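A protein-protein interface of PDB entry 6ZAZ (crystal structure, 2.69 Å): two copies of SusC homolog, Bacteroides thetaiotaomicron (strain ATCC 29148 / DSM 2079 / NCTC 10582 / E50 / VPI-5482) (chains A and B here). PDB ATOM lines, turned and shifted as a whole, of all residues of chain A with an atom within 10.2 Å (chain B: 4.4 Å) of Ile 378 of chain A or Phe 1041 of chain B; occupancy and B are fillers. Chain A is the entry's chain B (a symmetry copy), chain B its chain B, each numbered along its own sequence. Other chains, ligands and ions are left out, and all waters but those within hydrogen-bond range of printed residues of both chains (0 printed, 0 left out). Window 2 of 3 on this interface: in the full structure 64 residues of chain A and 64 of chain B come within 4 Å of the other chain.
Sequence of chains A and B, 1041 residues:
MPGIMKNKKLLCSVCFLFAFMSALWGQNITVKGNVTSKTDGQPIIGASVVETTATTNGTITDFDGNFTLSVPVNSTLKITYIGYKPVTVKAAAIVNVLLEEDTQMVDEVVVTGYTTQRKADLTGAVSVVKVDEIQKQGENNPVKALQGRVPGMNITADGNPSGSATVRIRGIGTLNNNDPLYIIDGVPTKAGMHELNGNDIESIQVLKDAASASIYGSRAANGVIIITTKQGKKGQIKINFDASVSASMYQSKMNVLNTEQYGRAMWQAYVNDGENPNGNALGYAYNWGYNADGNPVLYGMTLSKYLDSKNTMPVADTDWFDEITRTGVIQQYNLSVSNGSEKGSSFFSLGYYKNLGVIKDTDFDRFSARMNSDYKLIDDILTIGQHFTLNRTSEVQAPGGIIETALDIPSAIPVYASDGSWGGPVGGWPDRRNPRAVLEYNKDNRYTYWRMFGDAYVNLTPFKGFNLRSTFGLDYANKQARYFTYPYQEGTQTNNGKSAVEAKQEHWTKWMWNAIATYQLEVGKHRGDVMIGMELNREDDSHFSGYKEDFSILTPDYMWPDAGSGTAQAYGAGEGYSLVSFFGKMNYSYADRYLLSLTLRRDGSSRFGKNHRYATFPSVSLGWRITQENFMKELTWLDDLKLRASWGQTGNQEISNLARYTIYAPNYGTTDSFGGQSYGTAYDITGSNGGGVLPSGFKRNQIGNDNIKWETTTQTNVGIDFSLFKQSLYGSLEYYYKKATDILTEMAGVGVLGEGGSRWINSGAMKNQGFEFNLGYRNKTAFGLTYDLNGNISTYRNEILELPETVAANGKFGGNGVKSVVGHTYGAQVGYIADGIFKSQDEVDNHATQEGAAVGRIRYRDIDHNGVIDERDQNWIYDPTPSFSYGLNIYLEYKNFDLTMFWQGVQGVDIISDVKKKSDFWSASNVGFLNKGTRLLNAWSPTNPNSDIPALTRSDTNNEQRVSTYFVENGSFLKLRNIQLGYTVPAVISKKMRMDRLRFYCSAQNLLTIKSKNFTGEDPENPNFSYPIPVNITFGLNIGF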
ATOM      1  N   GLU A 342      -4.455   2.134  -5.895  1.00  0.00           N
ATOM      2  CA  GLU A 342      -4.971   1.713  -7.195  1.00  0.00           C
ATOM      3  C   GLU A 342      -4.635   2.735  -8.275  1.00  0.00           C
ATOM      4  O   GLU A 342      -4.329   2.377  -9.421  1.00  0.00           O
ATOM      5  CB  GLU A 342      -6.485   1.523  -7.087  1.00  0.00           C
ATOM      6  CG  GLU A 342      -7.128   2.621  -6.230  1.00  0.00           C
ATOM      7  CD  GLU A 342      -8.596   2.388  -5.940  1.00  0.00           C
ATOM      8  OE1 GLU A 342      -9.325   3.393  -5.755  1.00  0.00           O
ATOM      9  OE2 GLU A 342      -9.013   1.210  -5.889  1.00  0.00           O
ATOM     10  N   LYS A 343      -4.657   4.015  -7.907  1.00  0.00           N
ATOM     11  CA  LYS A 343      -4.536   5.127  -8.836  1.00  0.00           C
ATOM     12  C   LYS A 343      -3.103   5.612  -9.030  1.00  0.00           C
ATOM     13  O   LYS A 343      -2.828   6.271 -10.036  1.00  0.00           O
ATOM     14  CB  LYS A 343      -5.405   6.296  -8.349  1.00  0.00           C
ATOM     15  CG  LYS A 343      -6.903   6.057  -8.495  1.00  0.00           C
ATOM     16  CD  LYS A 343      -7.344   6.160  -9.959  1.00  0.00           C
ATOM     17  CE  LYS A 343      -8.860   6.068 -10.127  1.00  0.00           C
ATOM     18  NZ  LYS A 343      -9.280   4.765 -10.716  1.00  0.00           N
ATOM     19  N   TYR A 375       1.071   8.222 -11.713  1.00  0.00           N
ATOM     20  CA  TYR A 375      -0.342   8.551 -11.621  1.00  0.00           C
ATOM     21  C   TYR A 375      -1.064   7.944 -12.812  1.00  0.00           C
ATOM     22  O   TYR A 375      -0.651   8.167 -13.955  1.00  0.00           O
ATOM     23  CB  TYR A 375      -0.546  10.074 -11.597  1.00  0.00           C
ATOM     24  CG  TYR A 375       0.381  10.804 -10.650  1.00  0.00           C
ATOM     25  CD1 TYR A 375       1.714  11.006 -10.971  1.00  0.00           C
ATOM     26  CD2 TYR A 375      -0.077  11.297  -9.436  1.00  0.00           C
ATOM     27  CE1 TYR A 375       2.573  11.662 -10.105  1.00  0.00           C
ATOM     28  CE2 TYR A 375       0.780  11.962  -8.558  1.00  0.00           C
ATOM     29  CZ  TYR A 375       2.110  12.141  -8.903  1.00  0.00           C
ATOM     30  OH  TYR A 375       2.998  12.797  -8.069  1.00  0.00           O
ATOM     31  N   LYS A 376      -2.138   7.178 -12.540  1.00  0.00           N
ATOM     32  CA  LYS A 376      -2.961   6.520 -13.563  1.00  0.00           C
ATOM     33  C   LYS A 376      -4.295   7.251 -13.658  1.00  0.00           C
ATOM     34  O   LYS A 376      -5.100   7.199 -12.724  1.00  0.00           O
ATOM     35  CB  LYS A 376      -3.212   5.046 -13.243  1.00  0.00           C
ATOM     36  CG  LYS A 376      -2.119   4.328 -12.493  1.00  0.00           C
ATOM     37  CD  LYS A 376      -1.050   3.825 -13.435  1.00  0.00           C
ATOM     38  CE  LYS A 376      -0.025   2.993 -12.673  1.00  0.00           C
ATOM     39  NZ  LYS A 376      -0.685   1.943 -11.829  1.00  0.00           N
ATOM     40  N   LEU A 377      -4.542   7.896 -14.789  1.00  0.00           N
ATOM     41  CA  LEU A 377      -5.747   8.686 -14.998  1.00  0.00           C
ATOM     42  C   LEU A 377      -6.541   8.140 -16.180  1.00  0.00           C
ATOM     43  O   LEU A 377      -6.094   7.248 -16.915  1.00  0.00           O
ATOM     44  CB  LEU A 377      -5.397  10.159 -15.218  1.00  0.00           C
ATOM     45  CG  LEU A 377      -4.395  10.688 -14.191  1.00  0.00           C
ATOM     46  CD1 LEU A 377      -2.982  10.687 -14.755  1.00  0.00           C
ATOM     47  CD2 LEU A 377      -4.785  12.073 -13.733  1.00  0.00           C
ATOM     48  N   ILE A 378      -7.734   8.713 -16.355  1.00  0.00           N
ATOM     49  CA  ILE A 378      -8.747   8.187 -17.263  1.00  0.00           C
ATOM     50  C   ILE A 378      -9.051   6.747 -16.871  1.00  0.00           C
ATOM     51  O   ILE A 378      -9.714   6.505 -15.856  1.00  0.00           O
ATOM     52  CB  ILE A 378      -8.311   8.305 -18.731  1.00  0.00           C
ATOM     53  CG1 ILE A 378      -7.815   9.727 -18.991  1.00  0.00           C
ATOM     54  CG2 ILE A 378      -9.470   7.987 -19.647  1.00  0.00           C
ATOM     55  CD1 ILE A 378      -8.805  10.781 -18.631  1.00  0.00           C
ATOM     56  N   ASP A 379      -8.564   5.779 -17.640  1.00  0.00           N
ATOM     57  CA  ASP A 379      -8.882   4.378 -17.372  1.00  0.00           C
ATOM     58  C   ASP A 379      -7.615   3.547 -17.325  1.00  0.00           C
ATOM     59  O   ASP A 379      -7.517   2.470 -17.922  1.00  0.00           O
ATOM     60  CB  ASP A 379      -9.849   3.820 -18.415  1.00  0.00           C
ATOM     61  CG  ASP A 379     -11.250   4.390 -18.278  1.00  0.00           C
ATOM     62  OD1 ASP A 379     -11.717   4.573 -17.131  1.00  0.00           O
ATOM     63  OD2 ASP A 379     -11.885   4.648 -19.322  1.00  0.00           O
ATOM     64  N   ASP A 380      -6.629   4.038 -16.578  1.00  0.00           N
ATOM     65  CA  ASP A 380      -5.261   3.542 -16.680  1.00  0.00           C
ATOM     66  C   ASP A 380      -4.793   3.580 -18.130  1.00  0.00           C
ATOM     67  O   ASP A 380      -4.017   2.728 -18.574  1.00  0.00           O
ATOM     68  CB  ASP A 380      -5.124   2.134 -16.094  1.00  0.00           C
ATOM     69  CG  ASP A 380      -5.666   2.034 -14.683  1.00  0.00           C
ATOM     70  OD1 ASP A 380      -6.460   2.914 -14.283  1.00  0.00           O
ATOM     71  OD2 ASP A 380      -5.287   1.076 -13.973  1.00  0.00           O
ATOM     72  N   ILE A 381      -5.289   4.560 -18.884  1.00  0.00           N
ATOM     73  CA  ILE A 381      -4.884   4.745 -20.270  1.00  0.00           C
ATOM     74  C   ILE A 381      -4.085   6.027 -20.477  1.00  0.00           C
ATOM     75  O   ILE A 381      -3.379   6.143 -21.489  1.00  0.00           O
ATOM     76  CB  ILE A 381      -6.094   4.693 -21.232  1.00  0.00           C
ATOM     77  CG1 ILE A 381      -6.963   5.945 -21.120  1.00  0.00           C
ATOM     78  CG2 ILE A 381      -6.934   3.436 -20.983  1.00  0.00           C
ATOM     79  CD1 ILE A 381      -8.126   5.951 -22.107  1.00  0.00           C
ATOM     80  N   LEU A 382      -4.153   6.978 -19.560  1.00  0.00           N
ATOM     81  CA  LEU A 382      -3.185   8.065 -19.497  1.00  0.00           C
ATOM     82  C   LEU A 382      -2.388   7.902 -18.205  1.00  0.00           C
ATOM     83  O   LEU A 382      -2.966   7.885 -17.114  1.00  0.00           O
ATOM     84  CB  LEU A 382      -3.877   9.425 -19.557  1.00  0.00           C
ATOM     85  CG  LEU A 382      -3.009  10.619 -19.164  1.00  0.00           C
ATOM     86  CD1 LEU A 382      -1.725  10.704 -19.979  1.00  0.00           C
ATOM     87  CD2 LEU A 382      -3.810  11.883 -19.287  1.00  0.00           C
ATOM     88  N   THR A 383      -1.069   7.748 -18.332  1.00  0.00           N
ATOM     89  CA  THR A 383      -0.206   7.504 -17.183  1.00  0.00           C
ATOM     90  C   THR A 383       0.937   8.501 -17.188  1.00  0.00           C
ATOM     91  O   THR A 383       1.612   8.659 -18.206  1.00  0.00           O
ATOM     92  CB  THR A 383       0.352   6.080 -17.185  1.00  0.00           C
ATOM     93  OG1 THR A 383      -0.719   5.158 -16.975  1.00  0.00           O
ATOM     94  CG2 THR A 383       1.350   5.909 -16.060  1.00  0.00           C
ATOM     95  N   ILE A 384       1.149   9.173 -16.061  1.00  0.00           N
ATOM     96  CA  ILE A 384       2.259  10.100 -15.891  1.00  0.00           C
ATOM     97  C   ILE A 384       3.108   9.605 -14.736  1.00  0.00           C
ATOM     98  O   ILE A 384       2.583   9.071 -13.755  1.00  0.00           O
ATOM     99  CB  ILE A 384       1.788  11.544 -15.637  1.00  0.00           C
ATOM    100  CG1 ILE A 384       1.008  12.045 -16.844  1.00  0.00           C
ATOM    101  CG2 ILE A 384       2.972  12.458 -15.386  1.00  0.00           C
ATOM    102  CD1 ILE A 384       0.532  13.452 -16.692  1.00  0.00           C
ATOM    103  N   VAL A 458       5.358  10.496 -19.994  1.00  0.00           N
ATOM    104  CA  VAL A 458       3.934  10.294 -20.231  1.00  0.00           C
ATOM    105  C   VAL A 458       3.757   8.997 -21.009  1.00  0.00           C
ATOM    106  O   VAL A 458       4.548   8.688 -21.905  1.00  0.00           O
ATOM    107  CB  VAL A 458       3.295  11.476 -20.987  1.00  0.00           C
ATOM    108  CG1 VAL A 458       1.796  11.235 -21.172  1.00  0.00           C
ATOM    109  CG2 VAL A 458       3.550  12.773 -20.236  1.00  0.00           C
ATOM    110  N   ASN A 459       2.728   8.231 -20.657  1.00  0.00           N
ATOM    111  CA  ASN A 459       2.399   6.998 -21.354  1.00  0.00           C
ATOM    112  C   ASN A 459       0.925   7.005 -21.726  1.00  0.00           C
ATOM    113  O   ASN A 459       0.058   7.136 -20.855  1.00  0.00           O
ATOM    114  CB  ASN A 459       2.729   5.777 -20.502  1.00  0.00           C
ATOM    115  CG  ASN A 459       2.731   4.516 -21.313  1.00  0.00           C
ATOM    116  OD1 ASN A 459       3.770   4.087 -21.802  1.00  0.00           O
ATOM    117  ND2 ASN A 459       1.555   3.925 -21.493  1.00  0.00           N
ATOM    118  N   LEU A 460       0.652   6.856 -23.021  1.00  0.00           N
ATOM    119  CA  LEU A 460      -0.692   6.752 -23.572  1.00  0.00           C
ATOM    120  C   LEU A 460      -0.904   5.354 -24.138  1.00  0.00           C
ATOM    121  O   LEU A 460      -0.025   4.810 -24.820  1.00  0.00           O
ATOM    122  CB  LEU A 460      -0.906   7.786 -24.680  1.00  0.00           C
ATOM    123  CG  LEU A 460      -2.225   8.542 -24.685  1.00  0.00           C
ATOM    124  CD1 LEU A 460      -2.281   9.451 -23.485  1.00  0.00           C
ATOM    125  CD2 LEU A 460      -2.351   9.340 -25.952  1.00  0.00           C
ATOM    126  N   THR A 461      -2.070   4.774 -23.850  1.00  0.00           N
ATOM    127  CA  THR A 461      -2.490   3.495 -24.431  1.00  0.00           C
ATOM    128  C   THR A 461      -3.849   3.692 -25.094  1.00  0.00           C
ATOM    129  O   THR A 461      -4.893   3.445 -24.473  1.00  0.00           O
ATOM    130  CB  THR A 461      -2.556   2.394 -23.376  1.00  0.00           C
ATOM    131  OG1 THR A 461      -3.712   2.590 -22.560  1.00  0.00           O
ATOM    132  CG2 THR A 461      -1.335   2.420 -22.491  1.00  0.00           C
ATOM    133  N   PRO A 462      -3.877   4.110 -26.366  1.00  0.00           N
ATOM    134  CA  PRO A 462      -5.155   4.454 -27.018  1.00  0.00           C
ATOM    135  C   PRO A 462      -6.049   3.269 -27.372  1.00  0.00           C
ATOM    136  O   PRO A 462      -7.138   3.507 -27.902  1.00  0.00           O
ATOM    137  CB  PRO A 462      -4.714   5.192 -28.295  1.00  0.00           C
ATOM    138  CG  PRO A 462      -3.222   5.381 -28.179  1.00  0.00           C
ATOM    139  CD  PRO A 462      -2.731   4.306 -27.269  1.00  0.00           C
ATOM    140  N   ILE B 237      -7.864  11.951  -7.866  1.00  0.00           N
ATOM    141  CA  ILE B 237      -6.734  11.959  -8.798  1.00  0.00           C
ATOM    142  C   ILE B 237      -7.049  12.928  -9.939  1.00  0.00           C
ATOM    143  O   ILE B 237      -7.839  12.616 -10.837  1.00  0.00           O
ATOM    144  CB  ILE B 237      -6.396  10.552  -9.318  1.00  0.00           C
ATOM    145  CG1 ILE B 237      -5.167  10.592 -10.230  1.00  0.00           C
ATOM    146  CG2 ILE B 237      -7.608   9.857  -9.957  1.00  0.00           C
ATOM    147  CD1 ILE B 237      -4.182   9.492  -9.934  1.00  0.00           C
ATOM    148  N   LYS B 238      -6.442  14.117  -9.901  1.00  0.00           N
ATOM    149  CA  LYS B 238      -6.695  15.174 -10.872  1.00  0.00           C
ATOM    150  C   LYS B 238      -5.437  15.458 -11.682  1.00  0.00           C
ATOM    151  O   LYS B 238      -4.340  15.012 -11.352  1.00  0.00           O
ATOM    152  CB  LYS B 238      -7.175  16.465 -10.187  1.00  0.00           C
ATOM    153  CG  LYS B 238      -8.523  16.362  -9.455  1.00  0.00           C
ATOM    154  CD  LYS B 238      -9.672  15.933 -10.383  1.00  0.00           C
ATOM    155  CE  LYS B 238     -10.765  15.176  -9.628  1.00  0.00           C
ATOM    156  NZ  LYS B 238     -11.215  13.946 -10.357  1.00  0.00           N
ATOM    157  N   ILE B 239      -5.620  16.224 -12.757  1.00  0.00           N
ATOM    158  CA  ILE B 239      -4.522  16.716 -13.581  1.00  0.00           C
ATOM    159  C   ILE B 239      -4.945  18.072 -14.134  1.00  0.00           C
ATOM    160  O   ILE B 239      -6.139  18.351 -14.285  1.00  0.00           O
ATOM    161  CB  ILE B 239      -4.170  15.705 -14.689  1.00  0.00           C
ATOM    162  CG1 ILE B 239      -3.212  16.295 -15.713  1.00  0.00           C
ATOM    163  CG2 ILE B 239      -5.401  15.256 -15.381  1.00  0.00           C
ATOM    164  CD1 ILE B 239      -2.931  15.359 -16.852  1.00  0.00           C
ATOM    165  N   ARG B 994     -14.196  13.853 -21.507  1.00  0.00           N
ATOM    166  CA  ARG B 994     -13.551  13.556 -20.227  1.00  0.00           C
ATOM    167  C   ARG B 994     -12.684  14.732 -19.767  1.00  0.00           C
ATOM    168  O   ARG B 994     -11.454  14.687 -19.777  1.00  0.00           O
ATOM    169  CB  ARG B 994     -12.733  12.266 -20.303  1.00  0.00           C
ATOM    170  CG  ARG B 994     -13.448  11.095 -19.701  1.00  0.00           C
ATOM    171  CD  ARG B 994     -12.731   9.826 -20.029  1.00  0.00           C
ATOM    172  NE  ARG B 994     -13.222   8.718 -19.228  1.00  0.00           N
ATOM    173  CZ  ARG B 994     -13.158   7.451 -19.612  1.00  0.00           C
ATOM    174  NH1 ARG B 994     -12.624   7.141 -20.789  1.00  0.00           N
ATOM    175  NH2 ARG B 994     -13.627   6.496 -18.822  1.00  0.00           N
ATOM    176  N   MET B 995     -13.378  15.796 -19.355  1.00  0.00           N
ATOM    177  CA  MET B 995     -12.724  17.014 -18.877  1.00  0.00           C
ATOM    178  C   MET B 995     -13.666  17.642 -17.853  1.00  0.00           C
ATOM    179  O   MET B 995     -14.713  18.175 -18.231  1.00  0.00           O
ATOM    180  CB  MET B 995     -12.421  17.978 -20.021  1.00  0.00           C
ATOM    181  CG  MET B 995     -11.294  17.561 -20.961  1.00  0.00           C
ATOM    182  SD  MET B 995     -11.010  18.727 -22.322  1.00  0.00           S
ATOM    183  CE  MET B 995      -9.865  17.802 -23.345  1.00  0.00           C
ATOM    184  N   ASP B 996     -13.299  17.561 -16.565  1.00  0.00           N
ATOM    185  CA  ASP B 996     -14.075  18.243 -15.530  1.00  0.00           C
ATOM    186  C   ASP B 996     -14.252  19.712 -15.873  1.00  0.00           C
ATOM    187  O   ASP B 996     -15.300  20.309 -15.599  1.00  0.00           O
ATOM    188  CB  ASP B 996     -13.391  18.139 -14.165  1.00  0.00           C
ATOM    189  CG  ASP B 996     -12.930  16.741 -13.834  1.00  0.00           C
ATOM    190  OD1 ASP B 996     -12.393  16.062 -14.733  1.00  0.00           O
ATOM    191  OD2 ASP B 996     -13.078  16.336 -12.659  1.00  0.00           O
ATOM    192  N   ILE B1039      -7.177  23.178 -19.073  1.00  0.00           N
ATOM    193  CA  ILE B1039      -7.705  21.830 -19.255  1.00  0.00           C
ATOM    194  C   ILE B1039      -7.442  21.053 -17.984  1.00  0.00           C
ATOM    195  O   ILE B1039      -6.326  21.087 -17.455  1.00  0.00           O
ATOM    196  CB  ILE B1039      -7.066  21.091 -20.443  1.00  0.00           C
ATOM    197  CG1 ILE B1039      -7.403  21.764 -21.759  1.00  0.00           C
ATOM    198  CG2 ILE B1039      -7.552  19.659 -20.478  1.00  0.00           C
ATOM    199  CD1 ILE B1039      -6.455  21.385 -22.836  1.00  0.00           C
ATOM    200  N   GLY B1040      -8.457  20.343 -17.510  1.00  0.00           N
ATOM    201  CA  GLY B1040      -8.299  19.531 -16.326  1.00  0.00           C
ATOM    202  C   GLY B1040      -9.142  18.280 -16.374  1.00  0.00           C
ATOM    203  O   GLY B1040     -10.360  18.351 -16.563  1.00  0.00           O
ATOM    204  N   PHE B1041      -8.495  17.129 -16.225  1.00  0.00           N
ATOM    205  CA  PHE B1041      -9.185  15.850 -16.090  1.00  0.00           C
ATOM    206  C   PHE B1041      -9.285  15.524 -14.591  1.00  0.00           C
ATOM    207  O   PHE B1041      -9.171  16.420 -13.742  1.00  0.00           O
ATOM    208  CB  PHE B1041      -8.454  14.718 -16.826  1.00  0.00           C
ATOM    209  CG  PHE B1041      -8.200  14.972 -18.290  1.00  0.00           C
ATOM    210  CD1 PHE B1041      -7.427  16.044 -18.717  1.00  0.00           C
ATOM    211  CD2 PHE B1041      -8.689  14.098 -19.240  1.00  0.00           C
ATOM    212  CE1 PHE B1041      -7.186  16.261 -20.056  1.00  0.00           C
ATOM    213  CE2 PHE B1041      -8.453  14.310 -20.585  1.00  0.00           C
ATOM    214  CZ  PHE B1041      -7.697  15.394 -20.993  1.00  0.00           C
ATOM    215  OXT PHE B1041      -9.466  14.369 -14.183  1.00  0.00           O
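The backbone NH (N) of Lys 376 of chain A sits at hydrogen-bond distance from the backbone carbonyl oxygen (O) of Lys 343 of chain A.
The backbone NH (N) of Leu 377 of chain A is in hydrogen-bond range of the backbone carbonyl oxygen (O) of Leu 382 of chain A (2.8 Å).
The backbone carbonyl oxygen (O) of Ile 384 of chain A sits at hydrogen-bond distance from the backbone NH (N) of Tyr 375 of chain A.
O of Ile 239 of chain B lies within hydrogen-bond range of N of Phe 1041 of chain B.
OD2 of Asp 996 of chain B lies within salt-bridge range of NZ of Lys 238 of chain B, 3.8 Å away.
No position is printed for both chains.
Of the 9 pairs that touch across the chains among the printed residues, none has its exchanged pair printed and touching as well.
CD1 of Ile 237 of chain B touches O of Lys 343 of chain A, at 3.5 Å.
Ile 237 of chain B touches Lys 376 of chain A (CD1 to O, 3.7 Å).
CD2 of Leu 377 of chain A touches CG1 of Ile 237 of chain B (3.8 Å).
CD2 of Leu 377 of chain A touches O of Lys 238 of chain B, 3.8 Å away.
Leu 377 of chain A touches Ile 239 of chain B.
Arg 994 of chain B touches Ile 378 of chain A (NH1 to CG2, 3.5 Å).
Ile 378 of chain A touches Phe 1041 of chain B (CD1 to CD2, 3.4 Å).
CD1 of Ile 384 of chain A touches CD1 of Ile 239 of chain B, 3.96 Å away.
Hydrophobic or aromatic side chains of chain A that line the printed part of chain B: Leu 377, Ile 378 and Ile 384.
Among the printed residues, Asp or Glu carboxylates within 4 Å of a Lys or Arg side-chain nitrogen of the other chain: Asp 379 of chain A with Arg 994 of chain B (2.6 Å).
Tyr 375 of chain A touches none of the printed residues of chain B.
Of the printed residues of chain B, Lys 376 of chain A touches Ile 237.
Printed residues of chain B within 4 Å of Leu 377 of chain A: Ile 237 (3.8 Å), Lys 238 (3.8 Å) and Ile 239 (3.6 Å).
Of chain B, only Arg 994 (3.5 Å) and Phe 1041 (3.4 Å) come within 4 Å of Ile 378 of chain A.
Leu 460 of chain A touches none of the printed residues of chain B.
Of the printed residues of chain A, Ile 237 of chain B touches Lys 343 (3.5 Å), Lys 376 (3.7 Å) and Leu 377 (3.8 Å).
Lys 238 of chain B touches just one residue of chain A: Leu 377 (3.8 Å).
Of chain A, only Leu 377 (3.6 Å) and Ile 384 (3.96 Å) come within 4 Å of Ile 239 of chain B.
Of chain A, only Ile 378 (3.5 Å) and Asp 379 (2.6 Å) come within 4 Å of Arg 994 of chain B.
No residue of chain A comes within 4 Å of Gly 1040 of chain B.
Of chain A, only Ile 378 comes within 4 Å of Phe 1041 of chain B.
The nearest residue of chain A that does not touch Phe 1041 of chain B is Leu 377 of chain A (5.2 Å).
The nearest printed residue of chain B that does not touch Lys 343 of chain A is Lys 238 of chain B (8.0 Å).
The side-chain carboxylate (OD2) of Asp 379 of chain A lies within salt-bridge range of the guanidinium group (NH2) of Arg 994 of chain B, 2.6 Å away.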
